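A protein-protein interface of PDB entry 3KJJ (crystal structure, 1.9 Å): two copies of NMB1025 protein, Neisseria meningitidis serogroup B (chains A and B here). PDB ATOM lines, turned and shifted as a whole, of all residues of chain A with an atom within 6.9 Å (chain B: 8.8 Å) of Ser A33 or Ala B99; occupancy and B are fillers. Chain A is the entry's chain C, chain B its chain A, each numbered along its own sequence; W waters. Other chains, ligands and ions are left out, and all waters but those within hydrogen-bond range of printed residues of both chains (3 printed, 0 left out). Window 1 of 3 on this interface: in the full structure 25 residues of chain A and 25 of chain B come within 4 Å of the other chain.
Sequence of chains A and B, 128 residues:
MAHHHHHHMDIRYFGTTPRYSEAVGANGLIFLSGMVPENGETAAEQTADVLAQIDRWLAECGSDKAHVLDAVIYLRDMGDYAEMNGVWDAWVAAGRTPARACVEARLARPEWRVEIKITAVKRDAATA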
ATOM      1  N   TYR A  13       3.339 -18.755  19.649  1.00  0.00           N
ATOM      2  CA  TYR A  13       4.359 -18.237  18.732  1.00  0.00           C
ATOM      3  C   TYR A  13       4.474 -19.131  17.490  1.00  0.00           C
ATOM      4  O   TYR A  13       4.478 -20.360  17.603  1.00  0.00           O
ATOM      5  CB  TYR A  13       5.711 -18.116  19.444  1.00  0.00           C
ATOM      6  CG  TYR A  13       5.707 -17.185  20.650  1.00  0.00           C
ATOM      7  CD1 TYR A  13       6.052 -15.834  20.519  1.00  0.00           C
ATOM      8  CD2 TYR A  13       5.356 -17.656  21.917  1.00  0.00           C
ATOM      9  CE1 TYR A  13       6.046 -14.972  21.630  1.00  0.00           C
ATOM     10  CE2 TYR A  13       5.347 -16.810  23.027  1.00  0.00           C
ATOM     11  CZ  TYR A  13       5.689 -15.475  22.877  1.00  0.00           C
ATOM     12  OH  TYR A  13       5.679 -14.657  23.979  1.00  0.00           O
ATOM     13  N   ARG A  19      15.395 -13.796  16.545  1.00  0.00           N
ATOM     14  CA  ARG A  19      15.174 -12.355  16.406  1.00  0.00           C
ATOM     15  C   ARG A  19      13.697 -11.978  16.486  1.00  0.00           C
ATOM     16  O   ARG A  19      13.352 -10.918  17.011  1.00  0.00           O
ATOM     17  CB  ARG A  19      15.773 -11.861  15.073  1.00  0.00           C
ATOM     18  CG  ARG A  19      15.637 -10.351  14.817  1.00  0.00           C
ATOM     19  CD  ARG A  19      16.510  -9.918  13.651  1.00  0.00           C
ATOM     20  NE  ARG A  19      17.920 -10.158  13.951  1.00  0.00           N
ATOM     21  CZ  ARG A  19      18.902 -10.150  13.056  1.00  0.00           C
ATOM     22  NH1 ARG A  19      18.644  -9.932  11.772  1.00  0.00           N
ATOM     23  NH2 ARG A  19      20.145 -10.384  13.449  1.00  0.00           N
ATOM     24  N   TYR A  20      12.835 -12.857  15.979  1.00  0.00           N
ATOM     25  CA  TYR A  20      11.408 -12.574  15.850  1.00  0.00           C
ATOM     26  C   TYR A  20      10.628 -13.856  15.586  1.00  0.00           C
ATOM     27  O   TYR A  20      11.200 -14.889  15.225  1.00  0.00           O
ATOM     28  CB  TYR A  20      11.158 -11.581  14.695  1.00  0.00           C
ATOM     29  CG  TYR A  20      11.579 -12.110  13.343  1.00  0.00           C
ATOM     30  CD1 TYR A  20      10.751 -12.963  12.616  1.00  0.00           C
ATOM     31  CD2 TYR A  20      12.801 -11.746  12.784  1.00  0.00           C
ATOM     32  CE1 TYR A  20      11.137 -13.460  11.376  1.00  0.00           C
ATOM     33  CE2 TYR A  20      13.196 -12.230  11.537  1.00  0.00           C
ATOM     34  CZ  TYR A  20      12.362 -13.089  10.842  1.00  0.00           C
ATOM     35  OH  TYR A  20      12.743 -13.571   9.610  1.00  0.00           O
ATOM     36  N   SER A  21       9.316 -13.788  15.780  1.00  0.00           N
ATOM     37  CA  SER A  21       8.433 -14.836  15.290  1.00  0.00           C
ATOM     38  C   SER A  21       7.634 -14.262  14.135  1.00  0.00           C
ATOM     39  O   SER A  21       7.294 -13.071  14.117  1.00  0.00           O
ATOM     40  CB  SER A  21       7.487 -15.318  16.394  1.00  0.00           C
ATOM     41  OG  SER A  21       8.218 -15.726  17.534  1.00  0.00           O
ATOM     42  N   GLU A  22       7.330 -15.113  13.168  1.00  0.00           N
ATOM     43  CA  GLU A  22       6.575 -14.695  12.000  1.00  0.00           C
ATOM     44  C   GLU A  22       5.153 -14.318  12.394  1.00  0.00           C
ATOM     45  O   GLU A  22       4.574 -13.378  11.856  1.00  0.00           O
ATOM     46  CB  GLU A  22       6.578 -15.815  10.952  1.00  0.00           C
ATOM     47  CG  GLU A  22       7.966 -16.134  10.383  1.00  0.00           C
ATOM     48  CD  GLU A  22       8.478 -15.079   9.407  1.00  0.00           C
ATOM     49  OE1 GLU A  22       7.814 -14.031   9.213  1.00  0.00           O
ATOM     50  OE2 GLU A  22       9.558 -15.302   8.832  1.00  0.00           O
ATOM     51  N   ALA A  23       4.587 -15.054  13.341  1.00  0.00           N
ATOM     52  CA  ALA A  23       3.255 -14.738  13.828  1.00  0.00           C
ATOM     53  C   ALA A  23       3.180 -14.955  15.335  1.00  0.00           C
ATOM     54  O   ALA A  23       3.796 -15.873  15.868  1.00  0.00           O
ATOM     55  CB  ALA A  23       2.205 -15.567  13.098  1.00  0.00           C
ATOM     56  N   VAL A  24       2.442 -14.080  16.009  1.00  0.00           N
ATOM     57  CA  VAL A  24       2.198 -14.192  17.435  1.00  0.00           C
ATOM     58  C   VAL A  24       0.699 -14.046  17.666  1.00  0.00           C
ATOM     59  O   VAL A  24       0.092 -13.088  17.194  1.00  0.00           O
ATOM     60  CB  VAL A  24       2.997 -13.119  18.228  1.00  0.00           C
ATOM     61  CG1 VAL A  24       2.686 -13.176  19.707  1.00  0.00           C
ATOM     62  CG2 VAL A  24       4.505 -13.281  17.989  1.00  0.00           C
ATOM     63  N   PHE A  31      -0.696 -11.138  15.424  1.00  0.00           N
ATOM     64  CA  PHE A  31       0.259 -10.134  14.984  1.00  0.00           C
ATOM     65  C   PHE A  31       1.309 -10.778  14.113  1.00  0.00           C
ATOM     66  O   PHE A  31       2.065 -11.635  14.570  1.00  0.00           O
ATOM     67  CB  PHE A  31       0.906  -9.424  16.173  1.00  0.00           C
ATOM     68  CG  PHE A  31      -0.037  -8.537  16.926  1.00  0.00           C
ATOM     69  CD1 PHE A  31      -0.122  -7.181  16.626  1.00  0.00           C
ATOM     70  CD2 PHE A  31      -0.863  -9.060  17.912  1.00  0.00           C
ATOM     71  CE1 PHE A  31      -0.999  -6.348  17.317  1.00  0.00           C
ATOM     72  CE2 PHE A  31      -1.746  -8.236  18.607  1.00  0.00           C
ATOM     73  CZ  PHE A  31      -1.812  -6.880  18.307  1.00  0.00           C
ATOM     74  N   LEU A  32       1.345 -10.365  12.850  1.00  0.00           N
ATOM     75  CA  LEU A  32       2.344 -10.855  11.915  1.00  0.00           C
ATOM     76  C   LEU A  32       3.539  -9.914  11.903  1.00  0.00           C
ATOM     77  O   LEU A  32       3.373  -8.705  12.024  1.00  0.00           O
ATOM     78  CB  LEU A  32       1.762 -10.944  10.500  1.00  0.00           C
ATOM     79  CG  LEU A  32       0.593 -11.877  10.196  1.00  0.00           C
ATOM     80  CD1 LEU A  32       0.419 -11.971   8.683  1.00  0.00           C
ATOM     81  CD2 LEU A  32       0.834 -13.268  10.789  1.00  0.00           C
ATOM     82  N   SER A  33       4.734 -10.486  11.789  1.00  0.00           N
ATOM     83  CA  SER A  33       5.956  -9.731  11.527  1.00  0.00           C
ATOM     84  C   SER A  33       5.786  -9.012  10.196  1.00  0.00           C
ATOM     85  O   SER A  33       4.969  -9.419   9.366  1.00  0.00           O
ATOM     86  CB  SER A  33       7.172 -10.674  11.439  1.00  0.00           C
ATOM     87  OG  SER A  33       7.835 -10.830  12.685  1.00  0.00           O
ATOM     88  N   GLY A  34       6.550  -7.938   9.997  1.00  0.00           N
ATOM     89  CA  GLY A  34       6.650  -7.323   8.684  1.00  0.00           C
ATOM     90  C   GLY A  34       7.047  -8.390   7.683  1.00  0.00           C
ATOM     91  O   GLY A  34       8.086  -9.041   7.831  1.00  0.00           O
ATOM     92  N   MET A  35       6.196  -8.605   6.688  1.00  0.00           N
ATOM     93  CA  MET A  35       6.504  -9.570   5.642  1.00  0.00           C
ATOM     94  C   MET A  35       7.206  -8.816   4.522  1.00  0.00           C
ATOM     95  O   MET A  35       6.708  -7.795   4.023  1.00  0.00           O
ATOM     96  CB  MET A  35       5.241 -10.281   5.139  1.00  0.00           C
ATOM     97  CG  MET A  35       4.495 -11.109   6.197  1.00  0.00           C
ATOM     98  SD  MET A  35       5.412 -12.769   6.796  1.00  0.00           S
ATOM     99  CE  MET A  35       4.270 -13.203   8.309  1.00  0.00           C
ATOM    100  N   VAL A  36       8.373  -9.322   4.152  1.00  0.00           N
ATOM    101  CA  VAL A  36       9.204  -8.741   3.090  1.00  0.00           C
ATOM    102  C   VAL A  36       9.368  -9.710   1.905  1.00  0.00           C
ATOM    103  O   VAL A  36       9.173 -10.911   2.056  1.00  0.00           O
ATOM    104  CB  VAL A  36      10.594  -8.308   3.639  1.00  0.00           C
ATOM    105  CG1 VAL A  36      10.458  -7.090   4.534  1.00  0.00           C
ATOM    106  CG2 VAL A  36      11.279  -9.465   4.380  1.00  0.00           C
ATOM    107  N   ILE A  54       1.650 -13.719   3.658  1.00  0.00           N
ATOM    108  CA  ILE A  54       0.598 -13.324   4.587  1.00  0.00           C
ATOM    109  C   ILE A  54      -0.531 -14.360   4.612  1.00  0.00           C
ATOM    110  O   ILE A  54      -0.973 -14.765   5.691  1.00  0.00           O
ATOM    111  CB  ILE A  54       0.098 -11.880   4.283  1.00  0.00           C
ATOM    112  CG1 ILE A  54       1.161 -10.861   4.735  1.00  0.00           C
ATOM    113  CG2 ILE A  54      -1.238 -11.580   4.978  1.00  0.00           C
ATOM    114  CD1 ILE A  54       0.955  -9.467   4.199  1.00  0.00           C
ATOM    115  N   GLU A 115       7.046  -3.738   2.226  1.00  0.00           N
ATOM    116  CA  GLU A 115       6.891  -4.542   3.428  1.00  0.00           C
ATOM    117  C   GLU A 115       5.485  -4.309   3.969  1.00  0.00           C
ATOM    118  O   GLU A 115       5.025  -3.171   4.019  1.00  0.00           O
ATOM    119  CB  GLU A 115       7.952  -4.173   4.476  1.00  0.00           C
ATOM    120  CG  GLU A 115       7.845  -4.954   5.785  1.00  0.00           C
ATOM    121  CD  GLU A 115       9.058  -4.817   6.686  1.00  0.00           C
ATOM    122  OE1 GLU A 115      10.067  -4.218   6.265  1.00  0.00           O
ATOM    123  OE2 GLU A 115       9.016  -5.333   7.821  1.00  0.00           O
ATOM    124  N   ILE A 116       4.784  -5.389   4.316  1.00  0.00           N
ATOM    125  CA  ILE A 116       3.420  -5.266   4.830  1.00  0.00           C
ATOM    126  C   ILE A 116       3.286  -5.901   6.215  1.00  0.00           C
ATOM    127  O   ILE A 116       3.694  -7.048   6.422  1.00  0.00           O
ATOM    128  CB  ILE A 116       2.359  -5.814   3.846  1.00  0.00           C
ATOM    129  CG1 ILE A 116       2.449  -5.059   2.504  1.00  0.00           C
ATOM    130  CG2 ILE A 116       0.971  -5.680   4.441  1.00  0.00           C
ATOM    131  CD1 ILE A 116       1.574  -5.603   1.403  1.00  0.00           C
ATOM    132  N   LYS A 117       2.707  -5.128   7.131  1.00  0.00           N
ATOM    133  CA  LYS A 117       2.558  -5.525   8.522  1.00  0.00           C
ATOM    134  C   LYS A 117       1.084  -5.700   8.851  1.00  0.00           C
ATOM    135  O   LYS A 117       0.306  -4.768   8.754  1.00  0.00           O
ATOM    136  CB  LYS A 117       3.205  -4.480   9.436  1.00  0.00           C
ATOM    137  CG  LYS A 117       3.784  -5.064  10.700  1.00  0.00           C
ATOM    138  CD  LYS A 117       2.763  -5.082  11.804  1.00  0.00           C
ATOM    139  CE  LYS A 117       2.963  -3.928  12.763  1.00  0.00           C
ATOM    140  NZ  LYS A 117       2.139  -4.110  13.992  1.00  0.00           N
ATOM    141  N   ILE A 118       0.711  -6.917   9.236  1.00  0.00           N
ATOM    142  CA  ILE A 118      -0.690  -7.299   9.424  1.00  0.00           C
ATOM    143  C   ILE A 118      -1.047  -7.566  10.881  1.00  0.00           C
ATOM    144  O   ILE A 118      -0.252  -8.148  11.619  1.00  0.00           O
ATOM    145  CB  ILE A 118      -0.991  -8.583   8.584  1.00  0.00           C
ATOM    146  CG1 ILE A 118      -0.872  -8.299   7.084  1.00  0.00           C
ATOM    147  CG2 ILE A 118      -2.363  -9.217   8.936  1.00  0.00           C
ATOM    148  CD1 ILE A 118      -1.997  -7.439   6.507  1.00  0.00           C
ATOM    149  N   VAL B  68       5.940  -9.736  24.958  1.00  0.00           N
ATOM    150  CA  VAL B  68       5.775  -8.805  23.843  1.00  0.00           C
ATOM    151  C   VAL B  68       5.183  -9.545  22.652  1.00  0.00           C
ATOM    152  O   VAL B  68       5.662 -10.620  22.260  1.00  0.00           O
ATOM    153  CB  VAL B  68       7.109  -8.138  23.441  1.00  0.00           C
ATOM    154  CG1 VAL B  68       6.932  -7.249  22.218  1.00  0.00           C
ATOM    155  CG2 VAL B  68       7.666  -7.324  24.596  1.00  0.00           C
ATOM    156  N   LEU B  69       4.138  -8.950  22.083  1.00  0.00           N
ATOM    157  CA  LEU B  69       3.443  -9.488  20.927  1.00  0.00           C
ATOM    158  C   LEU B  69       4.111  -8.982  19.665  1.00  0.00           C
ATOM    159  O   LEU B  69       4.385  -9.745  18.733  1.00  0.00           O
ATOM    160  CB  LEU B  69       1.994  -8.987  20.916  1.00  0.00           C
ATOM    161  CG  LEU B  69       1.049  -9.491  22.010  1.00  0.00           C
ATOM    162  CD1 LEU B  69      -0.229  -8.703  22.017  1.00  0.00           C
ATOM    163  CD2 LEU B  69       0.761 -10.970  21.845  1.00  0.00           C
ATOM    164  N   ASP B  70       4.345  -7.678  19.644  1.00  0.00           N
ATOM    165  CA  ASP B  70       4.699  -6.985  18.418  1.00  0.00           C
ATOM    166  C   ASP B  70       5.656  -5.847  18.736  1.00  0.00           C
ATOM    167  O   ASP B  70       5.531  -5.177  19.764  1.00  0.00           O
ATOM    168  CB  ASP B  70       3.410  -6.470  17.756  1.00  0.00           C
ATOM    169  CG  ASP B  70       3.640  -5.878  16.389  1.00  0.00           C
ATOM    170  OD1 ASP B  70       4.036  -6.626  15.477  1.00  0.00           O
ATOM    171  OD2 ASP B  70       3.407  -4.662  16.224  1.00  0.00           O
ATOM    172  N   ALA B  71       6.627  -5.637  17.854  1.00  0.00           N
ATOM    173  CA  ALA B  71       7.566  -4.545  18.010  1.00  0.00           C
ATOM    174  C   ALA B  71       7.798  -3.893  16.652  1.00  0.00           C
ATOM    175  O   ALA B  71       8.083  -4.579  15.671  1.00  0.00           O
ATOM    176  CB  ALA B  71       8.867  -5.053  18.584  1.00  0.00           C
ATOM    177  N   VAL B  72       7.664  -2.569  16.602  1.00  0.00           N
ATOM    178  CA  VAL B  72       8.037  -1.817  15.405  1.00  0.00           C
ATOM    179  C   VAL B  72       9.283  -1.002  15.687  1.00  0.00           C
ATOM    180  O   VAL B  72       9.302  -0.186  16.613  1.00  0.00           O
ATOM    181  CB  VAL B  72       6.909  -0.889  14.913  1.00  0.00           C
ATOM    182  CG1 VAL B  72       7.316  -0.264  13.583  1.00  0.00           C
ATOM    183  CG2 VAL B  72       5.627  -1.667  14.748  1.00  0.00           C
ATOM    184  N   ILE B  73      10.328  -1.227  14.890  1.00  0.00           N
ATOM    185  CA  ILE B  73      11.592  -0.549  15.110  1.00  0.00           C
ATOM    186  C   ILE B  73      11.808   0.430  13.979  1.00  0.00           C
ATOM    187  O   ILE B  73      11.801   0.045  12.809  1.00  0.00           O
ATOM    188  CB  ILE B  73      12.783  -1.535  15.193  1.00  0.00           C
ATOM    189  CG1 ILE B  73      12.527  -2.606  16.256  1.00  0.00           C
ATOM    190  CG2 ILE B  73      14.094  -0.774  15.491  1.00  0.00           C
ATOM    191  CD1 ILE B  73      13.336  -3.868  16.045  1.00  0.00           C
ATOM    192  N   TRP B  88      19.380  -5.995  20.215  1.00  0.00           N
ATOM    193  CA  TRP B  88      18.057  -6.632  20.193  1.00  0.00           C
ATOM    194  C   TRP B  88      18.103  -8.149  20.372  1.00  0.00           C
ATOM    195  O   TRP B  88      17.358  -8.703  21.184  1.00  0.00           O
ATOM    196  CB  TRP B  88      17.343  -6.290  18.881  1.00  0.00           C
ATOM    197  CG  TRP B  88      16.037  -7.034  18.647  1.00  0.00           C
ATOM    198  CD1 TRP B  88      15.879  -8.231  17.998  1.00  0.00           C
ATOM    199  CD2 TRP B  88      14.722  -6.625  19.055  1.00  0.00           C
ATOM    200  NE1 TRP B  88      14.549  -8.585  17.976  1.00  0.00           N
ATOM    201  CE2 TRP B  88      13.820  -7.621  18.625  1.00  0.00           C
ATOM    202  CE3 TRP B  88      14.221  -5.518  19.757  1.00  0.00           C
ATOM    203  CZ2 TRP B  88      12.442  -7.544  18.870  1.00  0.00           C
ATOM    204  CZ3 TRP B  88      12.857  -5.439  19.996  1.00  0.00           C
ATOM    205  CH2 TRP B  88      11.982  -6.453  19.556  1.00  0.00           C
ATOM    206  N   VAL B  92      16.018 -10.043  23.550  1.00  0.00           N
ATOM    207  CA  VAL B  92      14.760 -10.790  23.403  1.00  0.00           C
ATOM    208  C   VAL B  92      14.721 -12.074  24.220  1.00  0.00           C
ATOM    209  O   VAL B  92      15.742 -12.733  24.404  1.00  0.00           O
ATOM    210  CB  VAL B  92      14.425 -11.134  21.928  1.00  0.00           C
ATOM    211  CG1 VAL B  92      13.984  -9.875  21.174  1.00  0.00           C
ATOM    212  CG2 VAL B  92      15.609 -11.841  21.235  1.00  0.00           C
ATOM    213  N   ARG B  96      10.550 -16.937  22.666  1.00  0.00           N
ATOM    214  CA  ARG B  96       9.336 -16.125  22.839  1.00  0.00           C
ATOM    215  C   ARG B  96       9.545 -14.733  22.245  1.00  0.00           C
ATOM    216  O   ARG B  96       9.252 -13.719  22.881  1.00  0.00           O
ATOM    217  CB  ARG B  96       8.968 -16.017  24.323  1.00  0.00           C
ATOM    218  CG  ARG B  96       8.480 -17.328  24.936  1.00  0.00           C
ATOM    219  CD  ARG B  96       8.027 -17.137  26.364  1.00  0.00           C
ATOM    220  NE  ARG B  96       6.838 -16.297  26.458  1.00  0.00           N
ATOM    221  CZ  ARG B  96       5.603 -16.750  26.664  1.00  0.00           C
ATOM    222  NH1 ARG B  96       5.376 -18.054  26.798  1.00  0.00           N
ATOM    223  NH2 ARG B  96       4.593 -15.893  26.739  1.00  0.00           N
ATOM    224  N   THR B  97      10.084 -14.701  21.029  1.00  0.00           N
ATOM    225  CA  THR B  97      10.453 -13.448  20.379  1.00  0.00           C
ATOM    226  C   THR B  97       9.255 -12.908  19.601  1.00  0.00           C
ATOM    227  O   THR B  97       8.516 -13.687  19.014  1.00  0.00           O
ATOM    228  CB  THR B  97      11.661 -13.651  19.438  1.00  0.00           C
ATOM    229  OG1 THR B  97      11.335 -14.634  18.451  1.00  0.00           O
ATOM    230  CG2 THR B  97      12.863 -14.142  20.214  1.00  0.00           C
ATOM    231  N   PRO B  98       9.057 -11.573  19.594  1.00  0.00           N
ATOM    232  CA  PRO B  98       7.805 -11.036  19.058  1.00  0.00           C
ATOM    233  C   PRO B  98       7.745 -10.913  17.539  1.00  0.00           C
ATOM    234  O   PRO B  98       8.744 -11.089  16.851  1.00  0.00           O
ATOM    235  CB  PRO B  98       7.723  -9.650  19.702  1.00  0.00           C
ATOM    236  CG  PRO B  98       9.175  -9.235  19.821  1.00  0.00           C
ATOM    237  CD  PRO B  98       9.931 -10.510  20.136  1.00  0.00           C
ATOM    238  N   ALA B  99       6.549 -10.635  17.033  1.00  0.00           N
ATOM    239  CA  ALA B  99       6.372 -10.157  15.671  1.00  0.00           C
ATOM    240  C   ALA B  99       7.177  -8.866  15.574  1.00  0.00           C
ATOM    241  O   ALA B  99       7.148  -8.028  16.487  1.00  0.00           O
ATOM    242  CB  ALA B  99       4.895  -9.888  15.394  1.00  0.00           C
ATOM    243  N   ARG B 100       7.926  -8.722  14.488  1.00  0.00           N
ATOM    244  CA  ARG B 100       8.792  -7.571  14.335  1.00  0.00           C
ATOM    245  C   ARG B 100       8.733  -6.999  12.936  1.00  0.00           C
ATOM    246  O   ARG B 100       8.612  -7.732  11.957  1.00  0.00           O
ATOM    247  CB  ARG B 100      10.246  -7.940  14.668  1.00  0.00           C
ATOM    248  CG  ARG B 100      11.086  -6.756  15.117  1.00  0.00           C
ATOM    249  CD  ARG B 100      12.539  -7.165  15.341  1.00  0.00           C
ATOM    250  NE  ARG B 100      13.312  -7.051  14.109  1.00  0.00           N
ATOM    251  CZ  ARG B 100      14.624  -6.866  14.048  1.00  0.00           C
ATOM    252  NH1 ARG B 100      15.356  -6.771  15.160  1.00  0.00           N
ATOM    253  NH2 ARG B 100      15.206  -6.778  12.863  1.00  0.00           N
ATOM    254  N   ALA B 101       8.833  -5.674  12.858  1.00  0.00           N
ATOM    255  CA  ALA B 101       9.147  -4.994  11.604  1.00  0.00           C
ATOM    256  C   ALA B 101      10.145  -3.882  11.885  1.00  0.00           C
ATOM    257  O   ALA B 101      10.064  -3.204  12.913  1.00  0.00           O
ATOM    258  CB  ALA B 101       7.894  -4.442  10.951  1.00  0.00           C
ATOM    259  N   CYS B 102      11.085  -3.698  10.962  1.00  0.00           N
ATOM    260  CA  CYS B 102      12.079  -2.654  11.090  1.00  0.00           C
ATOM    261  C   CYS B 102      12.128  -1.805   9.830  1.00  0.00           C
ATOM    262  O   CYS B 102      12.440  -2.311   8.757  1.00  0.00           O
ATOM    263  CB  CYS B 102      13.461  -3.262  11.364  1.00  0.00           C
ATOM    264  SG  CYS B 102      14.712  -1.991  11.508  1.00  0.00           S
ATOM    265  N   ILE B 116      11.568   2.400  19.405  1.00  0.00           N
ATOM    266  CA  ILE B 116      10.907   1.094  19.377  1.00  0.00           C
ATOM    267  C   ILE B 116       9.521   1.209  20.005  1.00  0.00           C
ATOM    268  O   ILE B 116       9.378   1.714  21.123  1.00  0.00           O
ATOM    269  CB  ILE B 116      11.751  -0.028  20.054  1.00  0.00           C
ATOM    270  CG1 ILE B 116      13.097  -0.209  19.339  1.00  0.00           C
ATOM    271  CG2 ILE B 116      10.998  -1.362  20.017  1.00  0.00           C
ATOM    272  CD1 ILE B 116      14.069  -1.099  20.065  1.00  0.00           C
ATOM    273  N   LYS B 117       8.520   0.751  19.253  1.00  0.00           N
ATOM    274  CA  LYS B 117       7.117   0.794  19.630  1.00  0.00           C
ATOM    275  C   LYS B 117       6.612  -0.630  19.866  1.00  0.00           C
ATOM    276  O   LYS B 117       6.688  -1.484  18.980  1.00  0.00           O
ATOM    277  CB  LYS B 117       6.317   1.493  18.518  1.00  0.00           C
ATOM    278  CG  LYS B 117       4.801   1.530  18.690  1.00  0.00           C
ATOM    279  CD  LYS B 117       4.106   0.475  17.826  1.00  0.00           C
ATOM    280  CE  LYS B 117       2.899   1.041  17.093  1.00  0.00           C
ATOM    281  NZ  LYS B 117       3.317   1.702  15.818  1.00  0.00           N
ATOM    282  N   ILE B 118       6.070  -0.859  21.058  1.00  0.00           N
ATOM    283  CA  ILE B 118       5.746  -2.203  21.535  1.00  0.00           C
ATOM    284  C   ILE B 118       4.252  -2.363  21.776  1.00  0.00           C
ATOM    285  O   ILE B 118       3.590  -1.451  22.283  1.00  0.00           O
ATOM    286  CB  ILE B 118       6.470  -2.482  22.888  1.00  0.00           C
ATOM    287  CG1 ILE B 118       7.987  -2.465  22.719  1.00  0.00           C
ATOM    288  CG2 ILE B 118       5.986  -3.794  23.535  1.00  0.00           C
ATOM    289  CD1 ILE B 118       8.551  -3.682  22.030  1.00  0.00           C
ATOM    290  N   THR B 119       3.739  -3.530  21.406  1.00  0.00           N
ATOM    291  CA  THR B 119       2.452  -4.014  21.892  1.00  0.00           C
ATOM    292  C   THR B 119       2.715  -5.266  22.722  1.00  0.00           C
ATOM    293  O   THR B 119       3.396  -6.191  22.269  1.00  0.00           O
ATOM    294  CB  THR B 119       1.478  -4.348  20.741  1.00  0.00           C
ATOM    295  OG1 THR B 119       1.350  -3.217  19.865  1.00  0.00           O
ATOM    296  CG2 THR B 119       0.088  -4.715  21.305  1.00  0.00           C
HETATM  297  O   HOH W   1       7.012 -12.492  23.740  1.00  0.00           O
HETATM  298  O   HOH W   2      12.835  -3.920   6.508  1.00  0.00           O
HETATM  299  O   HOH W   3      11.288  -5.842   9.009  1.00  0.00           O
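The side-chain amino group (NZ) of Lys A117 lies within salt-bridge range of the side-chain carboxylate (OD2) of Asp B70 (2.6 Å).
The indole nitrogen (NE1) of Trp B88 sits at hydrogen-bond distance from the backbone carbonyl oxygen (O) of Arg A19.
The side-chain hydroxyl (OH) of Tyr A13 is in hydrogen-bond range of the guanidinium group (NE) of Arg B96.
OG1 of Thr B97 lies close to O of Tyr A20 (3.2 Å).
O of Thr B97 sits at hydrogen-bond distance from OG of Ser A21 (2.5 Å).
The backbone carbonyl oxygen (O) of Pro B98 lies within hydrogen-bond range of the backbone NH (N) of Ser A21.
N of Arg B100 is in hydrogen-bond range of OG of Ser A33 (2.8 Å).
The backbone carbonyl oxygen (O) of Arg B100 sits at hydrogen-bond distance from the backbone NH (N) of Gly A34, 2.9 Å away.
The backbone carbonyl oxygen (O) of Thr B119 lies within hydrogen-bond range of the backbone NH (N) of Leu B69, at 2.9 Å.
The backbone NH (N) of Ala B71 sits at hydrogen-bond distance from the backbone carbonyl oxygen (O) of Ala B99 (2.8 Å).
The backbone NH of Ile B73 sits at hydrogen-bond distance from the backbone carbonyl oxygen of Ala B101, at 2.8 Å.
The backbone carbonyl oxygen of Ile B73 sits close to the side-chain sulfur of Cys B102 (3.8 Å).
The backbone NH (N) of Leu A32 lies within hydrogen-bond range of the backbone carbonyl oxygen (O) of Ile A118 (3.0 Å).
Arg B100 touches Arg A19.
CA of Tyr A20 touches O of Pro B98, at 3.2 Å.
Val A24 touches Leu B69.
N of Ala B99 touches CG2 of Val A24, at 3.5 Å.
Phe A31 touches Leu B69.
Phe A31 touches Asp B70 (CD1 to CB, 3.8 Å).
Phe A31 touches Ala B99.
Ala B99 touches Ser A33 (CA to OG, 3.4 Å).
CB of Ala B101 touches OE2 of Glu A115, at 3.4 Å.
O of Cys B102 touches OE1 of Glu A115, at 3.9 Å.
Of chain A, only Ser A21 (3.4 Å), Val A24 (3.5 Å), Phe A31 (3.4 Å), Leu A32 (3.7 Å) and Ser A33 (3.4 Å) come within 4 Å of Ala B99.
Gly A34 touches just these residues of chain B: Arg B100 and Ala B101.
Of the printed residues of chain B, Lys A117 touches Asp B70.
Of the printed residues of chain B, Phe A31 touches Leu B69 (3.8 Å), Asp B70 (3.8 Å) and Ala B99 (3.4 Å).
Of the printed residues of chain A, Pro B98 touches Tyr A20 and Ser A21.
The nearest residue of chain B that does not touch Ser A33 is Pro B98 (4.3 Å).
The nearest printed residue of chain A that does not touch Ala B99 is Tyr A20 (4.9 Å).
Hydrophobic or aromatic side chains of chain A within 4 Å of the printed part of chain B: Tyr A13, Tyr A20, Val A24 and Phe A31.
Of the 19 printed residues of chain B, 10 touch a printed residue of chain A.
Hydrophobic or aromatic side chains of chain B within 4 Å of the printed part of chain A: Leu B69, Trp B88, Ala B99 and Ala B101.
Along chain B the printed residues that touch a printed residue of chain A span positions 69 to 102.
Among the printed residues, 24 pairs touch across the chains.
Among the printed residues, Asp or Glu carboxylates within 4 Å of a Lys or Arg side-chain nitrogen of the other chain: Lys A117 with Asp B70.
3 positions are printed for both chains.
Of the 24 pairs that touch across the chains among the printed residues, none has its exchanged pair printed and touching as well.
Water W1 lies within hydrogen-bond range of OH of Tyr A13 (2.6 Å), O of Arg B96 (2.7 Å) and O of Val B68 (2.7 Å).
Water W3 bridges the side-chain carboxylate of Glu A115 and the backbone NH of Cys B102.
Water W2 lies within hydrogen-bond range of O of Cys B102 and OE1 of Glu A115.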
